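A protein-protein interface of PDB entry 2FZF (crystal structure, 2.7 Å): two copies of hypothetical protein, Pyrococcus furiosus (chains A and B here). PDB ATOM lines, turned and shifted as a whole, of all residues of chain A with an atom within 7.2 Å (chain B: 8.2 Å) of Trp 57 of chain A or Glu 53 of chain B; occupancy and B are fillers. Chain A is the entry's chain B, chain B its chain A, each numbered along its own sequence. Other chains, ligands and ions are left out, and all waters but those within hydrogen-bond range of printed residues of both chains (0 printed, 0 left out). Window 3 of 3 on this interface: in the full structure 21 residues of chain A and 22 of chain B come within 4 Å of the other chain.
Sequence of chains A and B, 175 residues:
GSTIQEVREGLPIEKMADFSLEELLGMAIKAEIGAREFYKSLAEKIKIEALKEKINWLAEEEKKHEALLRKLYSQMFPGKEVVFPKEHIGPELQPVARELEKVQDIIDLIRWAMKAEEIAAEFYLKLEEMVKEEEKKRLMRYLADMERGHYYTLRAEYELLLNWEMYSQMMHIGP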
ATOM      1  N   TYR A  39      -4.465  -8.007  13.799  1.00  0.00           N
ATOM      2  CA  TYR A  39      -5.212  -7.504  14.946  1.00  0.00           C
ATOM      3  C   TYR A  39      -6.479  -8.327  15.150  1.00  0.00           C
ATOM      4  O   TYR A  39      -6.942  -8.501  16.273  1.00  0.00           O
ATOM      5  CB  TYR A  39      -5.568  -6.027  14.727  1.00  0.00           C
ATOM      6  CG  TYR A  39      -4.423  -5.060  14.943  1.00  0.00           C
ATOM      7  CD1 TYR A  39      -4.304  -3.906  14.169  1.00  0.00           C
ATOM      8  CD2 TYR A  39      -3.496  -5.259  15.962  1.00  0.00           C
ATOM      9  CE1 TYR A  39      -3.290  -2.967  14.412  1.00  0.00           C
ATOM     10  CE2 TYR A  39      -2.482  -4.330  16.214  1.00  0.00           C
ATOM     11  CZ  TYR A  39      -2.385  -3.193  15.443  1.00  0.00           C
ATOM     12  OH  TYR A  39      -1.393  -2.277  15.710  1.00  0.00           O
ATOM     13  N   ALA A  43      -6.707 -10.287  18.799  1.00  0.00           N
ATOM     14  CA  ALA A  43      -7.840 -10.071  19.693  1.00  0.00           C
ATOM     15  C   ALA A  43      -8.654 -11.337  19.912  1.00  0.00           C
ATOM     16  O   ALA A  43      -9.226 -11.544  20.983  1.00  0.00           O
ATOM     17  CB  ALA A  43      -8.734  -8.976  19.132  1.00  0.00           C
ATOM     18  N   LEU A  51      -8.203  -5.646  27.006  1.00  0.00           N
ATOM     19  CA  LEU A  51      -7.251  -5.558  25.904  1.00  0.00           C
ATOM     20  C   LEU A  51      -7.940  -5.939  24.606  1.00  0.00           C
ATOM     21  O   LEU A  51      -7.804  -5.240  23.610  1.00  0.00           O
ATOM     22  CB  LEU A  51      -6.056  -6.493  26.141  1.00  0.00           C
ATOM     23  CG  LEU A  51      -5.010  -6.600  25.025  1.00  0.00           C
ATOM     24  CD1 LEU A  51      -4.372  -5.242  24.784  1.00  0.00           C
ATOM     25  CD2 LEU A  51      -3.941  -7.619  25.409  1.00  0.00           C
ATOM     26  N   LYS A  52      -8.680  -7.046  24.625  1.00  0.00           N
ATOM     27  CA  LYS A  52      -9.381  -7.525  23.437  1.00  0.00           C
ATOM     28  C   LYS A  52     -10.205  -6.412  22.792  1.00  0.00           C
ATOM     29  O   LYS A  52     -10.318  -6.348  21.568  1.00  0.00           O
ATOM     30  CB  LYS A  52     -10.284  -8.715  23.791  1.00  0.00           C
ATOM     31  CG  LYS A  52     -11.055  -9.293  22.608  1.00  0.00           C
ATOM     32  CD  LYS A  52     -12.206 -10.189  23.064  1.00  0.00           C
ATOM     33  CE  LYS A  52     -11.762 -11.617  23.350  1.00  0.00           C
ATOM     34  NZ  LYS A  52     -11.500 -12.394  22.103  1.00  0.00           N
ATOM     35  N   GLU A  53     -10.772  -5.527  23.608  1.00  0.00           N
ATOM     36  CA  GLU A  53     -11.564  -4.422  23.066  1.00  0.00           C
ATOM     37  C   GLU A  53     -10.699  -3.483  22.218  1.00  0.00           C
ATOM     38  O   GLU A  53     -10.959  -3.304  21.023  1.00  0.00           O
ATOM     39  CB  GLU A  53     -12.248  -3.641  24.201  1.00  0.00           C
ATOM     40  CG  GLU A  53     -13.341  -4.443  24.921  1.00  0.00           C
ATOM     41  CD  GLU A  53     -14.115  -3.631  25.951  1.00  0.00           C
ATOM     42  OE1 GLU A  53     -15.036  -4.201  26.589  1.00  0.00           O
ATOM     43  OE2 GLU A  53     -13.808  -2.429  26.126  1.00  0.00           O
ATOM     44  N   LYS A  54      -9.669  -2.904  22.840  1.00  0.00           N
ATOM     45  CA  LYS A  54      -8.756  -1.991  22.157  1.00  0.00           C
ATOM     46  C   LYS A  54      -8.232  -2.565  20.851  1.00  0.00           C
ATOM     47  O   LYS A  54      -8.190  -1.880  19.831  1.00  0.00           O
ATOM     48  CB  LYS A  54      -7.564  -1.633  23.055  1.00  0.00           C
ATOM     49  CG  LYS A  54      -7.911  -0.707  24.216  1.00  0.00           C
ATOM     50  CD  LYS A  54      -6.670  -0.120  24.892  1.00  0.00           C
ATOM     51  CE  LYS A  54      -7.052   0.779  26.072  1.00  0.00           C
ATOM     52  NZ  LYS A  54      -5.858   1.308  26.788  1.00  0.00           N
ATOM     53  N   ILE A  55      -7.831  -3.828  20.881  1.00  0.00           N
ATOM     54  CA  ILE A  55      -7.304  -4.457  19.684  1.00  0.00           C
ATOM     55  C   ILE A  55      -8.359  -4.579  18.601  1.00  0.00           C
ATOM     56  O   ILE A  55      -8.060  -4.415  17.420  1.00  0.00           O
ATOM     57  CB  ILE A  55      -6.755  -5.849  19.979  1.00  0.00           C
ATOM     58  CG1 ILE A  55      -5.709  -5.766  21.091  1.00  0.00           C
ATOM     59  CG2 ILE A  55      -6.158  -6.440  18.715  1.00  0.00           C
ATOM     60  CD1 ILE A  55      -4.554  -4.847  20.787  1.00  0.00           C
ATOM     61  N   ASN A  56      -9.591  -4.880  19.000  1.00  0.00           N
ATOM     62  CA  ASN A  56     -10.665  -5.018  18.031  1.00  0.00           C
ATOM     63  C   ASN A  56     -10.903  -3.685  17.336  1.00  0.00           C
ATOM     64  O   ASN A  56     -11.027  -3.625  16.111  1.00  0.00           O
ATOM     65  CB  ASN A  56     -11.951  -5.508  18.713  1.00  0.00           C
ATOM     66  CG  ASN A  56     -12.201  -7.006  18.500  1.00  0.00           C
ATOM     67  OD1 ASN A  56     -12.227  -7.499  17.364  1.00  0.00           O
ATOM     68  ND2 ASN A  56     -12.402  -7.731  19.599  1.00  0.00           N
ATOM     69  N   TRP A  57     -10.943  -2.611  18.114  1.00  0.00           N
ATOM     70  CA  TRP A  57     -11.164  -1.295  17.537  1.00  0.00           C
ATOM     71  C   TRP A  57     -10.028  -0.910  16.582  1.00  0.00           C
ATOM     72  O   TRP A  57     -10.231  -0.131  15.650  1.00  0.00           O
ATOM     73  CB  TRP A  57     -11.322  -0.256  18.645  1.00  0.00           C
ATOM     74  CG  TRP A  57     -11.542   1.120  18.111  1.00  0.00           C
ATOM     75  CD1 TRP A  57     -10.638   2.144  18.089  1.00  0.00           C
ATOM     76  CD2 TRP A  57     -12.733   1.621  17.485  1.00  0.00           C
ATOM     77  NE1 TRP A  57     -11.191   3.250  17.492  1.00  0.00           N
ATOM     78  CE2 TRP A  57     -12.476   2.958  17.111  1.00  0.00           C
ATOM     79  CE3 TRP A  57     -13.994   1.071  17.205  1.00  0.00           C
ATOM     80  CZ2 TRP A  57     -13.433   3.758  16.467  1.00  0.00           C
ATOM     81  CZ3 TRP A  57     -14.949   1.868  16.562  1.00  0.00           C
ATOM     82  CH2 TRP A  57     -14.659   3.197  16.204  1.00  0.00           C
ATOM     83  N   LEU A  58      -8.840  -1.466  16.805  1.00  0.00           N
ATOM     84  CA  LEU A  58      -7.709  -1.178  15.936  1.00  0.00           C
ATOM     85  C   LEU A  58      -7.852  -1.925  14.622  1.00  0.00           C
ATOM     86  O   LEU A  58      -7.368  -1.467  13.579  1.00  0.00           O
ATOM     87  CB  LEU A  58      -6.388  -1.564  16.599  1.00  0.00           C
ATOM     88  CG  LEU A  58      -5.990  -0.788  17.846  1.00  0.00           C
ATOM     89  CD1 LEU A  58      -4.609  -1.207  18.275  1.00  0.00           C
ATOM     90  CD2 LEU A  58      -6.013   0.679  17.574  1.00  0.00           C
ATOM     91  N   ALA A  59      -8.508  -3.078  14.665  1.00  0.00           N
ATOM     92  CA  ALA A  59      -8.709  -3.861  13.451  1.00  0.00           C
ATOM     93  C   ALA A  59      -9.612  -3.093  12.483  1.00  0.00           C
ATOM     94  O   ALA A  59      -9.369  -3.096  11.278  1.00  0.00           O
ATOM     95  CB  ALA A  59      -9.319  -5.208  13.789  1.00  0.00           C
ATOM     96  N   GLU A  60     -10.636  -2.425  13.020  1.00  0.00           N
ATOM     97  CA  GLU A  60     -11.574  -1.648  12.201  1.00  0.00           C
ATOM     98  C   GLU A  60     -10.880  -0.513  11.490  1.00  0.00           C
ATOM     99  O   GLU A  60     -11.116  -0.267  10.310  1.00  0.00           O
ATOM    100  CB  GLU A  60     -12.708  -1.072  13.060  1.00  0.00           C
ATOM    101  CG  GLU A  60     -13.270   0.300  12.589  1.00  0.00           C
ATOM    102  CD  GLU A  60     -13.854   0.306  11.163  1.00  0.00           C
ATOM    103  OE1 GLU A  60     -14.315   1.387  10.710  1.00  0.00           O
ATOM    104  OE2 GLU A  60     -13.854  -0.756  10.495  1.00  0.00           O
ATOM    105  N   GLU A  61     -10.036   0.192  12.229  1.00  0.00           N
ATOM    106  CA  GLU A  61      -9.301   1.310  11.676  1.00  0.00           C
ATOM    107  C   GLU A  61      -8.448   0.882  10.489  1.00  0.00           C
ATOM    108  O   GLU A  61      -8.344   1.608   9.505  1.00  0.00           O
ATOM    109  CB  GLU A  61      -8.438   1.933  12.766  1.00  0.00           C
ATOM    110  CG  GLU A  61      -9.271   2.637  13.826  1.00  0.00           C
ATOM    111  CD  GLU A  61      -9.873   3.933  13.311  1.00  0.00           C
ATOM    112  OE1 GLU A  61     -10.790   4.474  13.974  1.00  0.00           O
ATOM    113  OE2 GLU A  61      -9.414   4.417  12.246  1.00  0.00           O
ATOM    114  N   GLU A  62      -7.847  -0.301  10.580  1.00  0.00           N
ATOM    115  CA  GLU A  62      -7.010  -0.800   9.498  1.00  0.00           C
ATOM    116  C   GLU A  62      -7.870  -1.222   8.318  1.00  0.00           C
ATOM    117  O   GLU A  62      -7.401  -1.292   7.177  1.00  0.00           O
ATOM    118  CB  GLU A  62      -6.172  -1.988   9.971  1.00  0.00           C
ATOM    119  CG  GLU A  62      -5.344  -1.727  11.227  1.00  0.00           C
ATOM    120  CD  GLU A  62      -4.559  -0.424  11.168  1.00  0.00           C
ATOM    121  OE1 GLU A  62      -3.788  -0.216  10.209  1.00  0.00           O
ATOM    122  OE2 GLU A  62      -4.718   0.391  12.097  1.00  0.00           O
ATOM    123  N   MET A 146      -3.311   8.299  12.587  1.00  0.00           N
ATOM    124  CA  MET A 146      -3.977   7.128  13.112  1.00  0.00           C
ATOM    125  C   MET A 146      -2.936   6.100  13.555  1.00  0.00           C
ATOM    126  O   MET A 146      -3.049   5.517  14.632  1.00  0.00           O
ATOM    127  CB  MET A 146      -4.913   6.551  12.057  1.00  0.00           C
ATOM    128  CG  MET A 146      -6.148   7.414  11.809  1.00  0.00           C
ATOM    129  SD  MET A 146      -7.089   7.787  13.337  1.00  0.00           S
ATOM    130  CE  MET A 146      -7.291   6.131  14.042  1.00  0.00           C
ATOM    131  N   HIS A 150      -2.181   4.557  17.235  1.00  0.00           N
ATOM    132  CA  HIS A 150      -2.168   3.164  17.673  1.00  0.00           C
ATOM    133  C   HIS A 150      -0.902   2.850  18.455  1.00  0.00           C
ATOM    134  O   HIS A 150      -0.857   1.891  19.234  1.00  0.00           O
ATOM    135  CB  HIS A 150      -2.254   2.188  16.496  1.00  0.00           C
ATOM    136  CG  HIS A 150      -3.486   2.338  15.667  1.00  0.00           C
ATOM    137  ND1 HIS A 150      -4.609   3.001  16.117  1.00  0.00           N
ATOM    138  CD2 HIS A 150      -3.776   1.902  14.426  1.00  0.00           C
ATOM    139  CE1 HIS A 150      -5.539   2.965  15.181  1.00  0.00           C
ATOM    140  NE2 HIS A 150      -5.062   2.305  14.143  1.00  0.00           N
ATOM    141  N   THR A 153      -1.621   3.956  22.124  1.00  0.00           N
ATOM    142  CA  THR A 153      -2.667   3.074  22.619  1.00  0.00           C
ATOM    143  C   THR A 153      -2.049   1.729  23.027  1.00  0.00           C
ATOM    144  O   THR A 153      -2.316   1.210  24.113  1.00  0.00           O
ATOM    145  CB  THR A 153      -3.703   2.820  21.525  1.00  0.00           C
ATOM    146  OG1 THR A 153      -4.308   4.066  21.149  1.00  0.00           O
ATOM    147  CG2 THR A 153      -4.758   1.858  22.010  1.00  0.00           C
ATOM    148  N   ALA B  43     -20.541  14.031  20.434  1.00  0.00           N
ATOM    149  CA  ALA B  43     -21.063  12.917  19.650  1.00  0.00           C
ATOM    150  C   ALA B  43     -22.553  13.103  19.432  1.00  0.00           C
ATOM    151  O   ALA B  43     -23.044  12.973  18.316  1.00  0.00           O
ATOM    152  CB  ALA B  43     -20.793  11.597  20.354  1.00  0.00           C
ATOM    153  N   ILE B  46     -23.835  15.512  15.878  1.00  0.00           N
ATOM    154  CA  ILE B  46     -22.849  15.312  14.822  1.00  0.00           C
ATOM    155  C   ILE B  46     -23.509  14.959  13.496  1.00  0.00           C
ATOM    156  O   ILE B  46     -23.190  15.551  12.461  1.00  0.00           O
ATOM    157  CB  ILE B  46     -21.817  14.213  15.202  1.00  0.00           C
ATOM    158  CG1 ILE B  46     -20.775  14.770  16.185  1.00  0.00           C
ATOM    159  CG2 ILE B  46     -21.103  13.709  13.967  1.00  0.00           C
ATOM    160  CD1 ILE B  46     -19.877  15.847  15.620  1.00  0.00           C
ATOM    161  N   ILE B  48     -22.971  12.637  11.719  1.00  0.00           N
ATOM    162  CA  ILE B  48     -21.951  12.110  10.828  1.00  0.00           C
ATOM    163  C   ILE B  48     -21.582  10.703  11.260  1.00  0.00           C
ATOM    164  O   ILE B  48     -20.646  10.501  12.030  1.00  0.00           O
ATOM    165  CB  ILE B  48     -20.698  12.987  10.834  1.00  0.00           C
ATOM    166  CG1 ILE B  48     -21.081  14.416  10.443  1.00  0.00           C
ATOM    167  CG2 ILE B  48     -19.657  12.418   9.877  1.00  0.00           C
ATOM    168  CD1 ILE B  48     -19.910  15.361  10.252  1.00  0.00           C
ATOM    169  N   GLU B  49     -22.347   9.738  10.760  1.00  0.00           N
ATOM    170  CA  GLU B  49     -22.145   8.327  11.065  1.00  0.00           C
ATOM    171  C   GLU B  49     -20.710   7.879  10.785  1.00  0.00           C
ATOM    172  O   GLU B  49     -20.467   7.058   9.897  1.00  0.00           O
ATOM    173  CB  GLU B  49     -23.135   7.484  10.248  1.00  0.00           C
ATOM    174  CG  GLU B  49     -23.194   7.873   8.761  1.00  0.00           C
ATOM    175  CD  GLU B  49     -24.241   7.110   7.965  1.00  0.00           C
ATOM    176  OE1 GLU B  49     -25.442   7.187   8.316  1.00  0.00           O
ATOM    177  OE2 GLU B  49     -23.855   6.441   6.982  1.00  0.00           O
ATOM    178  N   ALA B  50     -19.763   8.415  11.547  1.00  0.00           N
ATOM    179  CA  ALA B  50     -18.360   8.065  11.378  1.00  0.00           C
ATOM    180  C   ALA B  50     -17.546   8.778  12.440  1.00  0.00           C
ATOM    181  O   ALA B  50     -16.804   8.160  13.202  1.00  0.00           O
ATOM    182  CB  ALA B  50     -17.878   8.475   9.992  1.00  0.00           C
ATOM    183  N   LEU B  51     -17.702  10.093  12.478  1.00  0.00           N
ATOM    184  CA  LEU B  51     -17.003  10.912  13.433  1.00  0.00           C
ATOM    185  C   LEU B  51     -17.651  10.740  14.802  1.00  0.00           C
ATOM    186  O   LEU B  51     -16.960  10.665  15.818  1.00  0.00           O
ATOM    187  CB  LEU B  51     -17.056  12.357  12.981  1.00  0.00           C
ATOM    188  CG  LEU B  51     -16.254  13.351  13.807  1.00  0.00           C
ATOM    189  CD1 LEU B  51     -14.786  12.942  13.889  1.00  0.00           C
ATOM    190  CD2 LEU B  51     -16.421  14.700  13.146  1.00  0.00           C
ATOM    191  N   LYS B  52     -18.982  10.667  14.815  1.00  0.00           N
ATOM    192  CA  LYS B  52     -19.749  10.465  16.045  1.00  0.00           C
ATOM    193  C   LYS B  52     -19.292   9.147  16.637  1.00  0.00           C
ATOM    194  O   LYS B  52     -19.337   8.947  17.850  1.00  0.00           O
ATOM    195  CB  LYS B  52     -21.253  10.385  15.741  1.00  0.00           C
ATOM    196  CG  LYS B  52     -22.143  10.091  16.965  1.00  0.00           C
ATOM    197  CD  LYS B  52     -23.590   9.759  16.577  1.00  0.00           C
ATOM    198  CE  LYS B  52     -24.348  10.962  16.017  1.00  0.00           C
ATOM    199  NZ  LYS B  52     -25.249  11.618  17.019  1.00  0.00           N
ATOM    200  N   GLU B  53     -18.863   8.245  15.753  1.00  0.00           N
ATOM    201  CA  GLU B  53     -18.369   6.918  16.129  1.00  0.00           C
ATOM    202  C   GLU B  53     -17.036   7.106  16.855  1.00  0.00           C
ATOM    203  O   GLU B  53     -16.864   6.637  17.982  1.00  0.00           O
ATOM    204  CB  GLU B  53     -18.156   6.047  14.875  1.00  0.00           C
ATOM    205  CG  GLU B  53     -19.004   4.753  14.778  1.00  0.00           C
ATOM    206  CD  GLU B  53     -18.636   3.667  15.804  1.00  0.00           C
ATOM    207  OE1 GLU B  53     -19.235   2.564  15.742  1.00  0.00           O
ATOM    208  OE2 GLU B  53     -17.758   3.901  16.674  1.00  0.00           O
ATOM    209  N   LYS B  54     -16.097   7.785  16.190  1.00  0.00           N
ATOM    210  CA  LYS B  54     -14.786   8.065  16.764  1.00  0.00           C
ATOM    211  C   LYS B  54     -14.991   8.845  18.047  1.00  0.00           C
ATOM    212  O   LYS B  54     -14.458   8.485  19.087  1.00  0.00           O
ATOM    213  CB  LYS B  54     -13.920   8.894  15.796  1.00  0.00           C
ATOM    214  CG  LYS B  54     -13.104   8.088  14.762  1.00  0.00           C
ATOM    215  CD  LYS B  54     -13.971   7.036  14.052  1.00  0.00           C
ATOM    216  CE  LYS B  54     -13.223   6.223  12.979  1.00  0.00           C
ATOM    217  NZ  LYS B  54     -12.865   6.996  11.747  1.00  0.00           N
ATOM    218  N   ILE B  55     -15.780   9.909  17.999  1.00  0.00           N
ATOM    219  CA  ILE B  55     -15.967  10.676  19.216  1.00  0.00           C
ATOM    220  C   ILE B  55     -16.613   9.890  20.341  1.00  0.00           C
ATOM    221  O   ILE B  55     -16.404  10.204  21.504  1.00  0.00           O
ATOM    222  CB  ILE B  55     -16.762  11.945  18.964  1.00  0.00           C
ATOM    223  CG1 ILE B  55     -15.979  12.837  18.004  1.00  0.00           C
ATOM    224  CG2 ILE B  55     -16.991  12.682  20.277  1.00  0.00           C
ATOM    225  CD1 ILE B  55     -14.622  13.239  18.522  1.00  0.00           C
ATOM    226  N   ASN B  56     -17.387   8.866  19.996  1.00  0.00           N
ATOM    227  CA  ASN B  56     -18.040   8.038  21.002  1.00  0.00           C
ATOM    228  C   ASN B  56     -17.079   7.025  21.640  1.00  0.00           C
ATOM    229  O   ASN B  56     -17.118   6.803  22.852  1.00  0.00           O
ATOM    230  CB  ASN B  56     -19.247   7.314  20.394  1.00  0.00           C
ATOM    231  CG  ASN B  56     -20.557   8.079  20.603  1.00  0.00           C
ATOM    232  OD1 ASN B  56     -20.838   8.554  21.710  1.00  0.00           O
ATOM    233  ND2 ASN B  56     -21.369   8.183  19.547  1.00  0.00           N
ATOM    234  N   TRP B  57     -16.214   6.414  20.834  1.00  0.00           N
ATOM    235  CA  TRP B  57     -15.258   5.445  21.360  1.00  0.00           C
ATOM    236  C   TRP B  57     -14.276   6.164  22.266  1.00  0.00           C
ATOM    237  O   TRP B  57     -13.824   5.634  23.281  1.00  0.00           O
ATOM    238  CB  TRP B  57     -14.481   4.772  20.228  1.00  0.00           C
ATOM    239  CG  TRP B  57     -13.416   3.838  20.735  1.00  0.00           C
ATOM    240  CD1 TRP B  57     -13.594   2.569  21.219  1.00  0.00           C
ATOM    241  CD2 TRP B  57     -12.017   4.123  20.866  1.00  0.00           C
ATOM    242  NE1 TRP B  57     -12.391   2.049  21.643  1.00  0.00           N
ATOM    243  CE2 TRP B  57     -11.407   2.982  21.438  1.00  0.00           C
ATOM    244  CE3 TRP B  57     -11.217   5.233  20.558  1.00  0.00           C
ATOM    245  CZ2 TRP B  57     -10.034   2.917  21.708  1.00  0.00           C
ATOM    246  CZ3 TRP B  57      -9.846   5.171  20.827  1.00  0.00           C
ATOM    247  CH2 TRP B  57      -9.272   4.018  21.396  1.00  0.00           C
ATOM    248  N   LEU B  58     -13.951   7.387  21.878  1.00  0.00           N
ATOM    249  CA  LEU B  58     -13.023   8.213  22.619  1.00  0.00           C
ATOM    250  C   LEU B  58     -13.638   8.608  23.961  1.00  0.00           C
ATOM    251  O   LEU B  58     -12.944   8.673  24.973  1.00  0.00           O
ATOM    252  CB  LEU B  58     -12.693   9.441  21.776  1.00  0.00           C
ATOM    253  CG  LEU B  58     -11.412  10.221  22.000  1.00  0.00           C
ATOM    254  CD1 LEU B  58     -11.247  11.188  20.851  1.00  0.00           C
ATOM    255  CD2 LEU B  58     -11.463  10.951  23.323  1.00  0.00           C
ATOM    256  N   ALA B  59     -14.941   8.861  23.975  1.00  0.00           N
ATOM    257  CA  ALA B  59     -15.626   9.241  25.212  1.00  0.00           C
ATOM    258  C   ALA B  59     -15.632   8.094  26.224  1.00  0.00           C
ATOM    259  O   ALA B  59     -15.457   8.309  27.428  1.00  0.00           O
ATOM    260  CB  ALA B  59     -17.058   9.665  24.908  1.00  0.00           C
ATOM    261  N   GLU B  60     -15.841   6.881  25.716  1.00  0.00           N
ATOM    262  CA  GLU B  60     -15.884   5.674  26.536  1.00  0.00           C
ATOM    263  C   GLU B  60     -14.526   5.404  27.147  1.00  0.00           C
ATOM    264  O   GLU B  60     -14.397   5.185  28.353  1.00  0.00           O
ATOM    265  CB  GLU B  60     -16.327   4.479  25.687  1.00  0.00           C
ATOM    266  CG  GLU B  60     -17.710   4.664  25.073  1.00  0.00           C
ATOM    267  CD  GLU B  60     -18.266   3.405  24.432  1.00  0.00           C
ATOM    268  OE1 GLU B  60     -18.405   2.383  25.146  1.00  0.00           O
ATOM    269  OE2 GLU B  60     -18.574   3.442  23.216  1.00  0.00           O
ATOM    270  N   GLU B  61     -13.513   5.420  26.291  1.00  0.00           N
ATOM    271  CA  GLU B  61     -12.139   5.197  26.714  1.00  0.00           C
ATOM    272  C   GLU B  61     -11.779   6.062  27.921  1.00  0.00           C
ATOM    273  O   GLU B  61     -11.200   5.569  28.883  1.00  0.00           O
ATOM    274  CB  GLU B  61     -11.194   5.509  25.556  1.00  0.00           C
ATOM    275  CG  GLU B  61     -10.899   4.329  24.659  1.00  0.00           C
ATOM    276  CD  GLU B  61      -9.944   3.355  25.313  1.00  0.00           C
ATOM    277  OE1 GLU B  61      -9.458   2.429  24.617  1.00  0.00           O
ATOM    278  OE2 GLU B  61      -9.674   3.518  26.529  1.00  0.00           O
ATOM    279  N   THR B 153      -5.441  10.762  17.292  1.00  0.00           N
ATOM    280  CA  THR B 153      -6.680  10.321  16.669  1.00  0.00           C
ATOM    281  C   THR B 153      -7.490  11.569  16.324  1.00  0.00           C
ATOM    282  O   THR B 153      -8.002  11.696  15.215  1.00  0.00           O
ATOM    283  CB  THR B 153      -7.513   9.421  17.621  1.00  0.00           C
ATOM    284  OG1 THR B 153      -6.723   8.301  18.029  1.00  0.00           O
ATOM    285  CG2 THR B 153      -8.769   8.914  16.931  1.00  0.00           C
ATOM    286  N   GLU B 157      -8.821  13.133  12.482  1.00  0.00           N
ATOM    287  CA  GLU B 157     -10.159  13.591  12.157  1.00  0.00           C
ATOM    288  C   GLU B 157     -10.112  15.021  11.625  1.00  0.00           C
ATOM    289  O   GLU B 157     -10.579  15.303  10.523  1.00  0.00           O
ATOM    290  CB  GLU B 157     -11.060  13.501  13.382  1.00  0.00           C
ATOM    291  CG  GLU B 157     -11.431  12.073  13.713  1.00  0.00           C
ATOM    292  CD  GLU B 157     -11.875  11.303  12.488  1.00  0.00           C
ATOM    293  OE1 GLU B 157     -12.632  11.867  11.664  1.00  0.00           O
ATOM    294  OE2 GLU B 157     -11.469  10.133  12.352  1.00  0.00           O
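Lys 54 of chain A touches Glu 61 of chain B, and with the chains exchanged Glu 61 of chain A touches Lys 54 of chain B. Trp 57 of chain A touches Glu 53 of chain B, but with the chains exchanged Glu 53 of chain A does not touch Trp 57 of chain B (5.6 Å). Trp 57 of chain B touches its own counterpart, Trp 57 of chain A. 13 positions are printed for both chains.
OE2 of Glu 157 of chain B lies within salt-bridge range of NZ of Lys 54 of chain B.
Printed residues of chain B within 4 Å of Lys 54 of chain A: Glu 61. Trp 57 of chain A touches two residues of chain B. Of the printed residues of chain B, Glu 61 of chain A touches Lys 54 (3.2 Å). Glu 53 of chain B touches just one residue of chain A: Trp 57. Printed residues of chain A within 4 Å of Lys 54 of chain B: Glu 61 (3.2 Å). Printed residues of chain A within 4 Å of Trp 57 of chain B: Trp 57 (3.5 Å). Printed residues of chain A within 4 Å of Glu 61 of chain B: Lys 54. The nearest residue of chain A that does not touch Glu 53 of chain B is Glu 60 of chain A (7.1 Å). The nearest printed residue of chain A that does not touch Trp 57 of chain B is Lys 54 of chain A (4.9 Å).
The side-chain amino group of Lys 54 of chain B is in salt-bridge range of the side-chain carboxylate of Glu 61 of chain A (3.95 Å).
OE1 of Glu 61 of chain B touches CE of Lys 54 of chain A (3.3 Å). Glu 53 of chain B touches Trp 57 of chain A (OE2 to CH2, 3.2 Å). Trp 57 of chain A touches Trp 57 of chain B (CD1 to CE2, 3.5 Å).
Of the 18 printed residues of chain B, 4 touch a printed residue of chain A. Printed residues of chain B that touch a printed residue of chain A: Glu 53, Lys 54, Trp 57 and Glu 61. Along chain B the printed residues that touch a printed residue of chain A span positions 53 to 61. Of the 17 printed residues of chain A, 3 touch a printed residue of chain B.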
